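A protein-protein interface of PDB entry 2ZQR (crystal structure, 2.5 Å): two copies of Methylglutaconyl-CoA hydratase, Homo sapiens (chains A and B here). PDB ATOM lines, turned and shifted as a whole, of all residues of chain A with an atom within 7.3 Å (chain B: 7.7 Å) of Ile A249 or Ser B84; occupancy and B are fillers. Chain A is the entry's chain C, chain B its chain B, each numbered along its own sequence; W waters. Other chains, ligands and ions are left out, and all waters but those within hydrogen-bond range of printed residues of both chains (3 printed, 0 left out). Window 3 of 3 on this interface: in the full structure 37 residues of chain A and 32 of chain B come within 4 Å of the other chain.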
ATOM      1  N   VAL A 217       9.838 -24.508  11.386  1.00  0.00           N
ATOM      2  CA  VAL A 217      11.220 -24.419  11.854  1.00  0.00           C
ATOM      3  C   VAL A 217      11.709 -25.785  12.328  1.00  0.00           C
ATOM      4  O   VAL A 217      12.863 -26.164  12.120  1.00  0.00           O
ATOM      5  CB  VAL A 217      11.370 -23.404  13.018  1.00  0.00           C
ATOM      6  CG1 VAL A 217      12.836 -23.278  13.413  1.00  0.00           C
ATOM      7  CG2 VAL A 217      10.813 -22.053  12.614  1.00  0.00           C
ATOM      8  N   GLU A 242      21.229 -31.854  19.197  1.00  0.00           N
ATOM      9  CA  GLU A 242      21.093 -30.889  20.290  1.00  0.00           C
ATOM     10  C   GLU A 242      21.024 -29.437  19.799  1.00  0.00           C
ATOM     11  O   GLU A 242      20.141 -28.679  20.205  1.00  0.00           O
ATOM     12  CB  GLU A 242      22.273 -31.059  21.261  1.00  0.00           C
ATOM     13  CG  GLU A 242      22.375 -30.044  22.390  1.00  0.00           C
ATOM     14  CD  GLU A 242      23.491 -30.395  23.368  1.00  0.00           C
ATOM     15  OE1 GLU A 242      23.193 -30.936  24.453  1.00  0.00           O
ATOM     16  OE2 GLU A 242      24.676 -30.152  23.056  1.00  0.00           O
ATOM     17  N   CYS A 244      20.325 -28.431  16.819  1.00  0.00           N
ATOM     18  CA  CYS A 244      19.184 -28.230  15.940  1.00  0.00           C
ATOM     19  C   CYS A 244      17.941 -28.042  16.807  1.00  0.00           C
ATOM     20  O   CYS A 244      17.120 -27.157  16.561  1.00  0.00           O
ATOM     21  CB  CYS A 244      19.012 -29.427  15.017  1.00  0.00           C
ATOM     22  SG  CYS A 244      20.172 -29.439  13.646  1.00  0.00           S
ATOM     23  N   TYR A 245      17.823 -28.869  17.837  1.00  0.00           N
ATOM     24  CA  TYR A 245      16.696 -28.802  18.759  1.00  0.00           C
ATOM     25  C   TYR A 245      16.630 -27.447  19.468  1.00  0.00           C
ATOM     26  O   TYR A 245      15.556 -26.862  19.603  1.00  0.00           O
ATOM     27  CB  TYR A 245      16.807 -29.908  19.813  1.00  0.00           C
ATOM     28  CG  TYR A 245      15.614 -29.973  20.732  1.00  0.00           C
ATOM     29  CD1 TYR A 245      14.464 -30.678  20.363  1.00  0.00           C
ATOM     30  CD2 TYR A 245      15.616 -29.308  21.954  1.00  0.00           C
ATOM     31  CE1 TYR A 245      13.348 -30.719  21.188  1.00  0.00           C
ATOM     32  CE2 TYR A 245      14.500 -29.339  22.790  1.00  0.00           C
ATOM     33  CZ  TYR A 245      13.370 -30.050  22.397  1.00  0.00           C
ATOM     34  OH  TYR A 245      12.264 -30.099  23.219  1.00  0.00           O
ATOM     35  N   ALA A 246      17.778 -26.968  19.939  1.00  0.00           N
ATOM     36  CA  ALA A 246      17.857 -25.680  20.630  1.00  0.00           C
ATOM     37  C   ALA A 246      17.165 -24.572  19.830  1.00  0.00           C
ATOM     38  O   ALA A 246      16.603 -23.629  20.411  1.00  0.00           O
ATOM     39  CB  ALA A 246      19.308 -25.306  20.866  1.00  0.00           C
ATOM     40  N   GLN A 247      17.204 -24.702  18.502  1.00  0.00           N
ATOM     41  CA  GLN A 247      16.603 -23.728  17.604  1.00  0.00           C
ATOM     42  C   GLN A 247      15.080 -23.730  17.621  1.00  0.00           C
ATOM     43  O   GLN A 247      14.456 -22.792  17.121  1.00  0.00           O
ATOM     44  CB  GLN A 247      17.098 -23.951  16.175  1.00  0.00           C
ATOM     45  CG  GLN A 247      18.590 -23.743  16.023  1.00  0.00           C
ATOM     46  CD  GLN A 247      19.052 -23.858  14.591  1.00  0.00           C
ATOM     47  OE1 GLN A 247      18.542 -23.172  13.698  1.00  0.00           O
ATOM     48  NE2 GLN A 247      20.027 -24.727  14.359  1.00  0.00           N
ATOM     49  N   THR A 248      14.477 -24.771  18.184  1.00  0.00           N
ATOM     50  CA  THR A 248      13.021 -24.830  18.248  1.00  0.00           C
ATOM     51  C   THR A 248      12.551 -24.354  19.615  1.00  0.00           C
ATOM     52  O   THR A 248      11.373 -24.034  19.807  1.00  0.00           O
ATOM     53  CB  THR A 248      12.477 -26.268  18.050  1.00  0.00           C
ATOM     54  OG1 THR A 248      12.820 -27.077  19.189  1.00  0.00           O
ATOM     55  CG2 THR A 248      13.043 -26.878  16.780  1.00  0.00           C
ATOM     56  N   ILE A 249      13.475 -24.294  20.563  1.00  0.00           N
ATOM     57  CA  ILE A 249      13.108 -23.895  21.906  1.00  0.00           C
ATOM     58  C   ILE A 249      12.498 -22.509  22.036  1.00  0.00           C
ATOM     59  O   ILE A 249      11.420 -22.362  22.606  1.00  0.00           O
ATOM     60  CB  ILE A 249      14.301 -24.014  22.882  1.00  0.00           C
ATOM     61  CG1 ILE A 249      14.715 -25.486  23.003  1.00  0.00           C
ATOM     62  CG2 ILE A 249      13.909 -23.455  24.256  1.00  0.00           C
ATOM     63  CD1 ILE A 249      15.738 -25.777  24.070  1.00  0.00           C
ATOM     64  N   PRO A 250      13.157 -21.478  21.493  1.00  0.00           N
ATOM     65  CA  PRO A 250      12.562 -20.148  21.643  1.00  0.00           C
ATOM     66  C   PRO A 250      11.583 -19.683  20.572  1.00  0.00           C
ATOM     67  O   PRO A 250      11.271 -18.493  20.502  1.00  0.00           O
ATOM     68  CB  PRO A 250      13.787 -19.249  21.743  1.00  0.00           C
ATOM     69  CG  PRO A 250      14.736 -19.898  20.770  1.00  0.00           C
ATOM     70  CD  PRO A 250      14.538 -21.392  20.976  1.00  0.00           C
ATOM     71  N   THR A 251      11.086 -20.602  19.749  1.00  0.00           N
ATOM     72  CA  THR A 251      10.144 -20.221  18.695  1.00  0.00           C
ATOM     73  C   THR A 251       8.716 -20.104  19.214  1.00  0.00           C
ATOM     74  O   THR A 251       8.358 -20.733  20.199  1.00  0.00           O
ATOM     75  CB  THR A 251      10.148 -21.233  17.527  1.00  0.00           C
ATOM     76  OG1 THR A 251       9.722 -22.520  18.000  1.00  0.00           O
ATOM     77  CG2 THR A 251      11.539 -21.335  16.924  1.00  0.00           C
ATOM     78  N   LYS A 252       7.904 -19.289  18.550  1.00  0.00           N
ATOM     79  CA  LYS A 252       6.516 -19.122  18.961  1.00  0.00           C
ATOM     80  C   LYS A 252       5.777 -20.431  18.734  1.00  0.00           C
ATOM     81  O   LYS A 252       4.962 -20.847  19.559  1.00  0.00           O
ATOM     82  CB  LYS A 252       5.825 -18.022  18.153  1.00  0.00           C
ATOM     83  CG  LYS A 252       6.466 -16.650  18.245  1.00  0.00           C
ATOM     84  CD  LYS A 252       5.614 -15.645  17.504  1.00  0.00           C
ATOM     85  CE  LYS A 252       6.355 -14.351  17.280  1.00  0.00           C
ATOM     86  NZ  LYS A 252       5.496 -13.363  16.568  1.00  0.00           N
ATOM     87  N   ARG A 254       6.601 -23.511  19.086  1.00  0.00           N
ATOM     88  CA  ARG A 254       6.709 -24.493  20.165  1.00  0.00           C
ATOM     89  C   ARG A 254       5.747 -24.193  21.306  1.00  0.00           C
ATOM     90  O   ARG A 254       5.260 -25.109  21.977  1.00  0.00           O
ATOM     91  CB  ARG A 254       8.131 -24.556  20.722  1.00  0.00           C
ATOM     92  CG  ARG A 254       8.321 -25.697  21.712  1.00  0.00           C
ATOM     93  CD  ARG A 254       9.711 -25.703  22.292  1.00  0.00           C
ATOM     94  NE  ARG A 254       9.956 -24.572  23.180  1.00  0.00           N
ATOM     95  CZ  ARG A 254       9.695 -24.571  24.483  1.00  0.00           C
ATOM     96  NH1 ARG A 254       9.176 -25.644  25.064  1.00  0.00           N
ATOM     97  NH2 ARG A 254       9.973 -23.501  25.212  1.00  0.00           N
ATOM     98  N   LEU A 255       5.494 -22.910  21.547  1.00  0.00           N
ATOM     99  CA  LEU A 255       4.559 -22.535  22.596  1.00  0.00           C
ATOM    100  C   LEU A 255       3.164 -22.855  22.049  1.00  0.00           C
ATOM    101  O   LEU A 255       2.339 -23.469  22.723  1.00  0.00           O
ATOM    102  CB  LEU A 255       4.672 -21.046  22.918  1.00  0.00           C
ATOM    103  CG  LEU A 255       6.013 -20.490  23.423  1.00  0.00           C
ATOM    104  CD1 LEU A 255       5.894 -18.976  23.539  1.00  0.00           C
ATOM    105  CD2 LEU A 255       6.397 -21.104  24.770  1.00  0.00           C
ATOM    106  N   ARG B  79       7.010 -30.199  31.178  1.00  0.00           N
ATOM    107  CA  ARG B  79       7.566 -29.309  30.172  1.00  0.00           C
ATOM    108  C   ARG B  79       6.828 -27.982  30.204  1.00  0.00           C
ATOM    109  O   ARG B  79       7.427 -26.920  30.068  1.00  0.00           O
ATOM    110  CB  ARG B  79       7.448 -29.942  28.782  1.00  0.00           C
ATOM    111  CG  ARG B  79       8.356 -29.316  27.731  1.00  0.00           C
ATOM    112  CD  ARG B  79       9.804 -29.343  28.197  1.00  0.00           C
ATOM    113  NE  ARG B  79      10.304 -30.701  28.407  1.00  0.00           N
ATOM    114  CZ  ARG B  79      10.732 -31.496  27.433  1.00  0.00           C
ATOM    115  NH1 ARG B  79      10.728 -31.069  26.175  1.00  0.00           N
ATOM    116  NH2 ARG B  79      11.163 -32.717  27.712  1.00  0.00           N
ATOM    117  N   LYS B  81       5.750 -26.518  32.602  1.00  0.00           N
ATOM    118  CA  LYS B  81       6.164 -25.746  33.775  1.00  0.00           C
ATOM    119  C   LYS B  81       7.652 -25.416  33.725  1.00  0.00           C
ATOM    120  O   LYS B  81       8.216 -24.914  34.700  1.00  0.00           O
ATOM    121  CB  LYS B  81       5.887 -26.517  35.072  1.00  0.00           C
ATOM    122  CG  LYS B  81       4.476 -27.061  35.216  1.00  0.00           C
ATOM    123  CD  LYS B  81       4.215 -27.496  36.656  1.00  0.00           C
ATOM    124  CE  LYS B  81       2.981 -28.381  36.769  1.00  0.00           C
ATOM    125  NZ  LYS B  81       3.238 -29.745  36.214  1.00  0.00           N
ATOM    126  N   MET B  82       8.292 -25.713  32.598  1.00  0.00           N
ATOM    127  CA  MET B  82       9.712 -25.438  32.461  1.00  0.00           C
ATOM    128  C   MET B  82       9.927 -24.137  31.709  1.00  0.00           C
ATOM    129  O   MET B  82       9.193 -23.814  30.775  1.00  0.00           O
ATOM    130  CB  MET B  82      10.413 -26.572  31.716  1.00  0.00           C
ATOM    131  CG  MET B  82      10.219 -27.943  32.325  1.00  0.00           C
ATOM    132  SD  MET B  82      11.268 -29.196  31.559  1.00  0.00           S
ATOM    133  CE  MET B  82      11.574 -30.293  32.954  1.00  0.00           C
ATOM    134  N   SER B  83      10.933 -23.384  32.135  1.00  0.00           N
ATOM    135  CA  SER B  83      11.263 -22.127  31.489  1.00  0.00           C
ATOM    136  C   SER B  83      12.106 -22.475  30.274  1.00  0.00           C
ATOM    137  O   SER B  83      12.731 -23.532  30.237  1.00  0.00           O
ATOM    138  CB  SER B  83      12.055 -21.243  32.448  1.00  0.00           C
ATOM    139  OG  SER B  83      13.184 -21.935  32.947  1.00  0.00           O
ATOM    140  N   SER B  84      12.126 -21.593  29.283  1.00  0.00           N
ATOM    141  CA  SER B  84      12.896 -21.842  28.068  1.00  0.00           C
ATOM    142  C   SER B  84      14.354 -22.197  28.371  1.00  0.00           C
ATOM    143  O   SER B  84      14.947 -23.045  27.701  1.00  0.00           O
ATOM    144  CB  SER B  84      12.844 -20.615  27.148  1.00  0.00           C
ATOM    145  OG  SER B  84      13.512 -19.511  27.739  1.00  0.00           O
ATOM    146  N   SER B  85      14.926 -21.549  29.380  1.00  0.00           N
ATOM    147  CA  SER B  85      16.315 -21.800  29.751  1.00  0.00           C
ATOM    148  C   SER B  85      16.494 -23.157  30.433  1.00  0.00           C
ATOM    149  O   SER B  85      17.619 -23.573  30.718  1.00  0.00           O
ATOM    150  CB  SER B  85      16.830 -20.686  30.672  1.00  0.00           C
ATOM    151  OG  SER B  85      16.171 -20.695  31.927  1.00  0.00           O
ATOM    152  N   GLU B  86      15.382 -23.841  30.688  1.00  0.00           N
ATOM    153  CA  GLU B  86      15.415 -25.151  31.348  1.00  0.00           C
ATOM    154  C   GLU B  86      15.257 -26.301  30.362  1.00  0.00           C
ATOM    155  O   GLU B  86      15.853 -27.364  30.533  1.00  0.00           O
ATOM    156  CB  GLU B  86      14.295 -25.258  32.392  1.00  0.00           C
ATOM    157  CG  GLU B  86      14.465 -24.407  33.637  1.00  0.00           C
ATOM    158  CD  GLU B  86      13.290 -24.550  34.583  1.00  0.00           C
ATOM    159  OE1 GLU B  86      13.052 -25.678  35.075  1.00  0.00           O
ATOM    160  OE2 GLU B  86      12.599 -23.537  34.827  1.00  0.00           O
ATOM    161  N   VAL B  87      14.439 -26.073  29.341  1.00  0.00           N
ATOM    162  CA  VAL B  87      14.152 -27.073  28.324  1.00  0.00           C
ATOM    163  C   VAL B  87      15.395 -27.703  27.707  1.00  0.00           C
ATOM    164  O   VAL B  87      15.559 -28.918  27.764  1.00  0.00           O
ATOM    165  CB  VAL B  87      13.255 -26.471  27.207  1.00  0.00           C
ATOM    166  CG1 VAL B  87      13.042 -27.484  26.089  1.00  0.00           C
ATOM    167  CG2 VAL B  87      11.912 -26.063  27.798  1.00  0.00           C
ATOM    168  N   GLY B  88      16.265 -26.883  27.127  1.00  0.00           N
ATOM    169  CA  GLY B  88      17.473 -27.411  26.515  1.00  0.00           C
ATOM    170  C   GLY B  88      18.226 -28.403  27.387  1.00  0.00           C
ATOM    171  O   GLY B  88      18.417 -29.559  26.998  1.00  0.00           O
ATOM    172  N   PRO B  89      18.660 -27.982  28.586  1.00  0.00           N
ATOM    173  CA  PRO B  89      19.399 -28.842  29.514  1.00  0.00           C
ATOM    174  C   PRO B  89      18.649 -30.116  29.868  1.00  0.00           C
ATOM    175  O   PRO B  89      19.247 -31.185  29.966  1.00  0.00           O
ATOM    176  CB  PRO B  89      19.600 -27.941  30.731  1.00  0.00           C
ATOM    177  CG  PRO B  89      19.631 -26.580  30.146  1.00  0.00           C
ATOM    178  CD  PRO B  89      18.495 -26.635  29.157  1.00  0.00           C
ATOM    179  N   PHE B  90      17.338 -29.999  30.062  1.00  0.00           N
ATOM    180  CA  PHE B  90      16.537 -31.162  30.417  1.00  0.00           C
ATOM    181  C   PHE B  90      16.510 -32.206  29.311  1.00  0.00           C
ATOM    182  O   PHE B  90      16.695 -33.394  29.564  1.00  0.00           O
ATOM    183  CB  PHE B  90      15.102 -30.772  30.748  1.00  0.00           C
ATOM    184  CG  PHE B  90      14.273 -31.932  31.226  1.00  0.00           C
ATOM    185  CD1 PHE B  90      14.459 -32.453  32.503  1.00  0.00           C
ATOM    186  CD2 PHE B  90      13.347 -32.543  30.383  1.00  0.00           C
ATOM    187  CE1 PHE B  90      13.734 -33.570  32.933  1.00  0.00           C
ATOM    188  CE2 PHE B  90      12.621 -33.658  30.804  1.00  0.00           C
ATOM    189  CZ  PHE B  90      12.814 -34.172  32.081  1.00  0.00           C
ATOM    190  N   VAL B  91      16.266 -31.764  28.083  1.00  0.00           N
ATOM    191  CA  VAL B  91      16.219 -32.685  26.962  1.00  0.00           C
ATOM    192  C   VAL B  91      17.581 -33.326  26.750  1.00  0.00           C
ATOM    193  O   VAL B  91      17.674 -34.490  26.349  1.00  0.00           O
ATOM    194  CB  VAL B  91      15.784 -31.974  25.674  1.00  0.00           C
ATOM    195  CG1 VAL B  91      15.908 -32.919  24.493  1.00  0.00           C
ATOM    196  CG2 VAL B  91      14.346 -31.501  25.809  1.00  0.00           C
ATOM    197  N   SER B  92      18.632 -32.565  27.030  1.00  0.00           N
ATOM    198  CA  SER B  92      19.990 -33.056  26.878  1.00  0.00           C
ATOM    199  C   SER B  92      20.293 -34.117  27.930  1.00  0.00           C
ATOM    200  O   SER B  92      21.090 -35.023  27.704  1.00  0.00           O
ATOM    201  CB  SER B  92      20.968 -31.893  26.986  1.00  0.00           C
ATOM    202  OG  SER B  92      20.772 -30.998  25.903  1.00  0.00           O
ATOM    203  N   ALA B 146       5.957 -28.833  16.923  1.00  0.00           N
ATOM    204  CA  ALA B 146       6.880 -27.758  16.577  1.00  0.00           C
ATOM    205  C   ALA B 146       8.330 -27.968  17.057  1.00  0.00           C
ATOM    206  O   ALA B 146       9.142 -27.029  17.031  1.00  0.00           O
ATOM    207  CB  ALA B 146       6.337 -26.421  17.098  1.00  0.00           C
ATOM    208  N   ILE B 147       8.662 -29.186  17.489  1.00  0.00           N
ATOM    209  CA  ILE B 147      10.033 -29.485  17.928  1.00  0.00           C
ATOM    210  C   ILE B 147      10.568 -30.711  17.203  1.00  0.00           C
ATOM    211  O   ILE B 147      10.003 -31.130  16.194  1.00  0.00           O
ATOM    212  CB  ILE B 147      10.098 -29.752  19.422  1.00  0.00           C
ATOM    213  CG1 ILE B 147       9.166 -30.915  19.765  1.00  0.00           C
ATOM    214  CG2 ILE B 147       9.742 -28.492  20.171  1.00  0.00           C
ATOM    215  CD1 ILE B 147       9.236 -31.365  21.186  1.00  0.00           C
HETATM  216  O   HOH W   1      22.881 -34.155  25.661  1.00  0.00           O
HETATM  217  O   HOH W   2       9.902 -28.533  25.056  1.00  0.00           O
HETATM  218  O   HOH W   3       9.428 -24.555  16.039  1.00  0.00           O
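Of the 13 printed residues of chain A, 5 touch a printed residue of chain B. Printed residues of chain A that touch a printed residue of chain B: Glu A242, Tyr A245, Thr A248, Ile A249 and Arg A254. Of the 15 printed residues of chain B, 8 touch a printed residue of chain A. Among the printed residues, 13 pairs touch across the chains.
OG of Ser B92 is in hydrogen-bond range of O of Gly B88. O of Thr A248 lies within hydrogen-bond range of OG1 of Thr A251, 2.9 Å away. The side-chain sulfur of Met B82 lies within hydrogen-bond range of the guanidinium group of Arg B79, 3.6 Å away. The backbone NH (N) of Arg A254 sits at hydrogen-bond distance from the side-chain hydroxyl (OG1) of Thr A251, 3.4 Å away. The backbone carbonyl oxygen (O) of Ile A249 sits at hydrogen-bond distance from the guanidinium group (NE) of Arg A254, 2.7 Å away. The backbone carbonyl oxygen (O) of Tyr A245 sits at hydrogen-bond distance from the side-chain hydroxyl (OG1) of Thr A248.
Printed residues of chain B within 4 Å of Glu A242: Ser B92 (2.8 Å). Cys A244 touches none of the printed residues of chain B. Of chain B, only Ser B84 (3.6 Å), Val B87 (3.8 Å) and Gly B88 (3.3 Å) come within 4 Å of Ile A249. Of the printed residues of chain B, Arg A254 touches Val B87 (3.9 Å), Ala B146 (3.5 Å) and Ile B147 (3.5 Å). Ser B83 touches none of the printed residues of chain A. Of chain A, only Ile A249 (3.6 Å) comes within 4 Å of Ser B84. Of the printed residues of chain A, Ser B92 touches Glu A242. The nearest residue of chain A that does not touch Ser B84 is Arg A254 (4.4 Å). The nearest printed residue of chain A that does not touch Ile B147 is Ile A249 (5.6 Å).
No position is printed for both chains. Of the 13 pairs that touch across the chains among the printed residues, none has its exchanged pair printed and touching as well.
Water W3 lies within hydrogen-bond range of the backbone carbonyl oxygen (O) of Ala B146 (2.7 Å) and the side-chain hydroxyl (OG1) of Thr A251 (2.8 Å). Water W1 lies within hydrogen-bond range of O of Ser B92 (2.9 Å) and OE1 of Glu A242 (3.5 Å). Water W2 lies within hydrogen-bond range of the guanidinium group (NH1) of Arg B79 (2.9 Å), the guanidinium group (NH1) of Arg A254 (3.0 Å) and the side-chain hydroxyl (OH) of Tyr A245 (3.4 Å).
Among the printed residues, merely in contact across the chains: Ile A249 with Gly B88 (3.3 Å), Arg A254 with Ile B147 (3.5 Å), Thr A248 with Ile B147 (3.5 Å), Arg A254 with Ala B146 (3.5 Å), Thr A248 with Ala B146 (3.6 Å), Tyr A245 with Val B91 (3.6 Å), Ile A249 with Ser B84 (3.6 Å), Ile A249 with Val B87 (3.8 Å), Tyr A245 with Ile B147 (3.8 Å), Arg A254 with Val B87 (3.9 Å) and Tyr A245 with Val B87 (3.96 Å).
OH of Tyr A245 sits at hydrogen-bond distance from NH1 of Arg B79 (3.5 Å). OE1 of Glu A242 lies within hydrogen-bond range of OG of Ser B92 (2.8 Å).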
